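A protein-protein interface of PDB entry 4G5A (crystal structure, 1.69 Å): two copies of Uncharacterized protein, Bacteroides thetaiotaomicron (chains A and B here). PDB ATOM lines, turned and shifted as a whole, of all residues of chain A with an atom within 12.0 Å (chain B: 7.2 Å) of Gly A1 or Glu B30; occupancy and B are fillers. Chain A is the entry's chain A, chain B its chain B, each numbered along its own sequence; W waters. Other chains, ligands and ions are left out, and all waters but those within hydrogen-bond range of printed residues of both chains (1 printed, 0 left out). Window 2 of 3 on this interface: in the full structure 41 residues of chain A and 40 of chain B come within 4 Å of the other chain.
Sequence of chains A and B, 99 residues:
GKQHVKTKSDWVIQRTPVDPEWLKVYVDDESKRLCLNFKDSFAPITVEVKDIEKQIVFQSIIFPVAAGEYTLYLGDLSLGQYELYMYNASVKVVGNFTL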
ATOM      1  N   GLY A   1      27.704  12.885  25.018  1.00  0.00           N
ATOM      2  CA  GLY A   1      27.435  11.439  24.743  1.00  0.00           C
ATOM      3  C   GLY A   1      27.186  10.691  26.041  1.00  0.00           C
ATOM      4  O   GLY A   1      26.933  11.326  27.064  1.00  0.00           O
ATOM      5  N   LYS A   2      27.272   9.358  26.006  1.00  0.00           N
ATOM      6  CA  LYS A   2      26.930   8.509  27.173  1.00  0.00           C
ATOM      7  C   LYS A   2      28.079   8.265  28.159  1.00  0.00           C
ATOM      8  O   LYS A   2      29.124   7.721  27.821  1.00  0.00           O
ATOM      9  CB  LYS A   2      26.401   7.184  26.686  1.00  0.00           C
ATOM     10  CG  LYS A   2      25.880   6.250  27.755  1.00  0.00           C
ATOM     11  CD  LYS A   2      25.752   4.843  27.162  1.00  0.00           C
ATOM     12  CE  LYS A   2      24.810   3.934  27.936  1.00  0.00           C
ATOM     13  NZ  LYS A   2      23.415   3.933  27.400  1.00  0.00           N
ATOM     14  N   GLN A   3      27.852   8.611  29.413  1.00  0.00           N
ATOM     15  CA  GLN A   3      28.889   8.535  30.412  1.00  0.00           C
ATOM     16  C   GLN A   3      28.394   7.752  31.629  1.00  0.00           C
ATOM     17  O   GLN A   3      27.289   7.989  32.088  1.00  0.00           O
ATOM     18  CB  GLN A   3      29.271   9.938  30.830  1.00  0.00           C
ATOM     19  CG  GLN A   3      30.422   9.968  31.787  1.00  0.00           C
ATOM     20  CD  GLN A   3      31.432  11.004  31.424  1.00  0.00           C
ATOM     21  OE1 GLN A   3      31.143  12.196  31.458  1.00  0.00           O
ATOM     22  NE2 GLN A   3      32.630  10.559  31.040  1.00  0.00           N
ATOM     23  N   HIS A   4      29.219   6.840  32.131  1.00  0.00           N
ATOM     24  CA  HIS A   4      29.000   6.168  33.432  1.00  0.00           C
ATOM     25  C   HIS A   4      28.980   7.182  34.554  1.00  0.00           C
ATOM     26  O   HIS A   4      29.819   8.077  34.640  1.00  0.00           O
ATOM     27  CB  HIS A   4      30.100   5.124  33.715  1.00  0.00           C
ATOM     28  CG  HIS A   4      29.883   4.311  34.972  1.00  0.00           C
ATOM     29  ND1 HIS A   4      30.777   4.316  36.024  1.00  0.00           N
ATOM     30  CD2 HIS A   4      28.894   3.451  35.322  1.00  0.00           C
ATOM     31  CE1 HIS A   4      30.341   3.503  36.974  1.00  0.00           C
ATOM     32  NE2 HIS A   4      29.199   2.968  36.575  1.00  0.00           N
ATOM     33  N   VAL A   5      27.973   7.058  35.415  1.00  0.00           N
ATOM     34  CA  VAL A   5      27.904   7.885  36.612  1.00  0.00           C
ATOM     35  C   VAL A   5      28.378   6.995  37.746  1.00  0.00           C
ATOM     36  O   VAL A   5      27.803   5.953  37.952  1.00  0.00           O
ATOM     37  CB  VAL A   5      26.447   8.333  36.889  1.00  0.00           C
ATOM     38  CG1 VAL A   5      26.334   9.041  38.254  1.00  0.00           C
ATOM     39  CG2 VAL A   5      25.898   9.192  35.727  1.00  0.00           C
ATOM     40  N   VAL B  27      24.547   8.642  31.974  1.00  0.00           N
ATOM     41  CA  VAL B  27      23.833   9.832  31.557  1.00  0.00           C
ATOM     42  C   VAL B  27      24.293  10.177  30.147  1.00  0.00           C
ATOM     43  O   VAL B  27      25.480  10.117  29.848  1.00  0.00           O
ATOM     44  CB  VAL B  27      24.053  11.035  32.524  1.00  0.00           C
ATOM     45  CG1 VAL B  27      25.531  11.393  32.639  1.00  0.00           C
ATOM     46  CG2 VAL B  27      23.229  12.248  32.079  1.00  0.00           C
ATOM     47  N   ASP B  28      23.329  10.502  29.301  1.00  0.00           N
ATOM     48  CA  ASP B  28      23.591  11.003  27.965  1.00  0.00           C
ATOM     49  C   ASP B  28      23.197  12.484  27.976  1.00  0.00           C
ATOM     50  O   ASP B  28      22.009  12.813  28.031  1.00  0.00           O
ATOM     51  CB  ASP B  28      22.774  10.237  26.945  1.00  0.00           C
ATOM     52  CG  ASP B  28      23.124  10.628  25.506  1.00  0.00           C
ATOM     53  OD1 ASP B  28      23.434  11.806  25.260  1.00  0.00           O
ATOM     54  OD2 ASP B  28      23.084   9.743  24.632  1.00  0.00           O
ATOM     55  N   ASP B  29      24.193  13.363  27.963  1.00  0.00           N
ATOM     56  CA  ASP B  29      23.946  14.814  28.043  1.00  0.00           C
ATOM     57  C   ASP B  29      23.418  15.412  26.742  1.00  0.00           C
ATOM     58  O   ASP B  29      22.927  16.527  26.744  1.00  0.00           O
ATOM     59  CB  ASP B  29      25.190  15.576  28.521  1.00  0.00           C
ATOM     60  CG  ASP B  29      26.399  15.396  27.607  1.00  0.00           C
ATOM     61  OD1 ASP B  29      26.276  14.812  26.503  1.00  0.00           O
ATOM     62  OD2 ASP B  29      27.486  15.843  28.024  1.00  0.00           O
ATOM     63  N   GLU B  30      23.484  14.675  25.641  1.00  0.00           N
ATOM     64  CA  GLU B  30      22.901  15.175  24.399  1.00  0.00           C
ATOM     65  C   GLU B  30      21.393  14.971  24.379  1.00  0.00           C
ATOM     66  O   GLU B  30      20.637  15.894  24.064  1.00  0.00           O
ATOM     67  CB  GLU B  30      23.557  14.496  23.202  1.00  0.00           C
ATOM     68  CG  GLU B  30      25.028  14.858  23.103  1.00  0.00           C
ATOM     69  CD  GLU B  30      25.666  14.359  21.831  1.00  0.00           C
ATOM     70  OE1 GLU B  30      26.114  15.220  21.042  1.00  0.00           O
ATOM     71  OE2 GLU B  30      25.712  13.118  21.622  1.00  0.00           O
ATOM     72  N   SER B  31      20.966  13.759  24.711  1.00  0.00           N
ATOM     73  CA  SER B  31      19.552  13.415  24.748  1.00  0.00           C
ATOM     74  C   SER B  31      18.885  13.759  26.105  1.00  0.00           C
ATOM     75  O   SER B  31      17.651  13.695  26.223  1.00  0.00           O
ATOM     76  CB  SER B  31      19.393  11.939  24.391  1.00  0.00           C
ATOM     77  OG  SER B  31      19.914  11.097  25.406  1.00  0.00           O
ATOM     78  N   LYS B  32      19.692  14.158  27.094  1.00  0.00           N
ATOM     79  CA  LYS B  32      19.246  14.447  28.476  1.00  0.00           C
ATOM     80  C   LYS B  32      18.478  13.248  29.035  1.00  0.00           C
ATOM     81  O   LYS B  32      17.354  13.382  29.532  1.00  0.00           O
ATOM     82  CB  LYS B  32      18.414  15.729  28.575  1.00  0.00           C
ATOM     83  CG  LYS B  32      19.175  17.029  28.258  1.00  0.00           C
ATOM     84  CD  LYS B  32      18.333  18.242  28.649  1.00  0.00           C
ATOM     85  CE  LYS B  32      19.162  19.496  28.811  1.00  0.00           C
ATOM     86  NZ  LYS B  32      18.250  20.656  28.912  1.00  0.00           N
ATOM     87  N   ARG B  33      19.107  12.078  28.923  1.00  0.00           N
ATOM     88  CA  ARG B  33      18.568  10.819  29.401  1.00  0.00           C
ATOM     89  C   ARG B  33      19.471  10.229  30.491  1.00  0.00           C
ATOM     90  O   ARG B  33      20.708  10.243  30.397  1.00  0.00           O
ATOM     91  CB  ARG B  33      18.426   9.800  28.255  1.00  0.00           C
ATOM     92  CG  ARG B  33      17.229  10.053  27.343  1.00  0.00           C
ATOM     93  CD  ARG B  33      17.362   9.270  26.055  1.00  0.00           C
ATOM     94  NE  ARG B  33      16.122   9.143  25.282  1.00  0.00           N
ATOM     95  CZ  ARG B  33      15.506  10.125  24.617  1.00  0.00           C
ATOM     96  NH1 ARG B  33      15.951  11.379  24.639  1.00  0.00           N
ATOM     97  NH2 ARG B  33      14.399   9.847  23.933  1.00  0.00           N
ATOM     98  N   TYR B  73      13.835  10.537  31.254  1.00  0.00           N
ATOM     99  CA  TYR B  73      14.042  11.720  30.435  1.00  0.00           C
ATOM    100  C   TYR B  73      14.128  12.968  31.291  1.00  0.00           C
ATOM    101  O   TYR B  73      13.195  13.285  32.040  1.00  0.00           O
ATOM    102  CB  TYR B  73      12.911  11.862  29.428  1.00  0.00           C
ATOM    103  CG  TYR B  73      13.045  13.082  28.544  1.00  0.00           C
ATOM    104  CD1 TYR B  73      14.241  13.367  27.875  1.00  0.00           C
ATOM    105  CD2 TYR B  73      11.968  13.931  28.356  1.00  0.00           C
ATOM    106  CE1 TYR B  73      14.348  14.468  27.065  1.00  0.00           C
ATOM    107  CE2 TYR B  73      12.064  15.023  27.553  1.00  0.00           C
ATOM    108  CZ  TYR B  73      13.254  15.302  26.904  1.00  0.00           C
ATOM    109  OH  TYR B  73      13.328  16.408  26.078  1.00  0.00           O
ATOM    110  N   LEU B  99      24.900  17.837  33.127  1.00  0.00           N
ATOM    111  CA  LEU B  99      24.224  17.986  31.848  1.00  0.00           C
ATOM    112  C   LEU B  99      24.848  19.198  31.152  1.00  0.00           C
ATOM    113  O   LEU B  99      25.188  20.223  31.782  1.00  0.00           O
ATOM    114  CB  LEU B  99      22.722  18.191  32.011  1.00  0.00           C
ATOM    115  CG  LEU B  99      21.915  17.002  32.478  1.00  0.00           C
ATOM    116  CD1 LEU B  99      20.401  17.366  32.593  1.00  0.00           C
ATOM    117  CD2 LEU B  99      22.133  15.787  31.577  1.00  0.00           C
ATOM    118  OXT LEU B  99      25.060  19.124  29.926  1.00  0.00           O
HETATM  119  O   HOH W   1      26.907  12.622  29.136  1.00  0.00           O
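Water W1 lies within hydrogen-bond range of O of Gly A1 (2.4 Å), O of Val B27 (3.0 Å) and N of Asp B29 (3.0 Å).
N of Gly A1 is in hydrogen-bond range of OD1 of Asp B29 (2.8 Å).
The backbone NH (N) of Val B27 lies within hydrogen-bond range of the backbone carbonyl oxygen (O) of Gln A3, 2.8 Å away.
The backbone carbonyl oxygen (O) of Gly A1 sits close to the backbone carbonyl oxygen (O) of Val B27 (3.4 Å).
The side-chain carboxylate of Asp B28 is in hydrogen-bond range of the backbone NH of Glu B30 (2.9 Å).
OD1 of Asp B28 lies within hydrogen-bond range of N of Ser B31, 3.2 Å away.
The backbone NH (N) of Asp B28 sits at hydrogen-bond distance from the backbone carbonyl oxygen (O) of Arg B33, at 2.9 Å.
Asp B28 touches Gly A1 (CA to O, 3.5 Å).
Gly A1 touches Glu B30 (N to CG, 3.8 Å).
Val B27 touches Lys A2 (O to CA, 3.4 Å).
Val B27 touches Val A5.
Of the 9 printed residues of chain B, 4 touch a printed residue of chain A.
Printed residues of chain B that touch a printed residue of chain A: Val B27, Asp B28, Asp B29 and Glu B30.
Hydrophobic or aromatic side chains of chain B within 4 Å of the printed part of chain A: Val B27.
Among the printed residues, 7 pairs touch across the chains.
Among the printed residues, no Asp or Glu carboxylate lies within 4 Å of a Lys or Arg side-chain nitrogen of the other chain.
No position is printed for both chains.
Of the 7 pairs that touch across the chains among the printed residues, none has its exchanged pair printed and touching as well.
Of the printed residues of chain B, Gly A1 touches Val B27, Asp B28, Asp B29 and Glu B30.
Of the printed residues of chain B, Lys A2 touches Val B27 (3.4 Å).
Of the printed residues of chain B, Gln A3 touches Val B27.
Printed residues of chain B within 4 Å of Val A5: Val B27 (3.8 Å).
Of the printed residues of chain A, Val B27 touches Gly A1 (3.4 Å), Lys A2 (3.4 Å), Gln A3 (2.8 Å) and Val A5 (3.8 Å).
Of chain A, only Gly A1 comes within 4 Å of Asp B28.
No residue of chain A comes within 4 Å of Ser B31.
Leu B99 touches none of the printed residues of chain A.
The nearest printed residue of chain B that does not touch Gly A1 is Ser B31 (6.8 Å).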
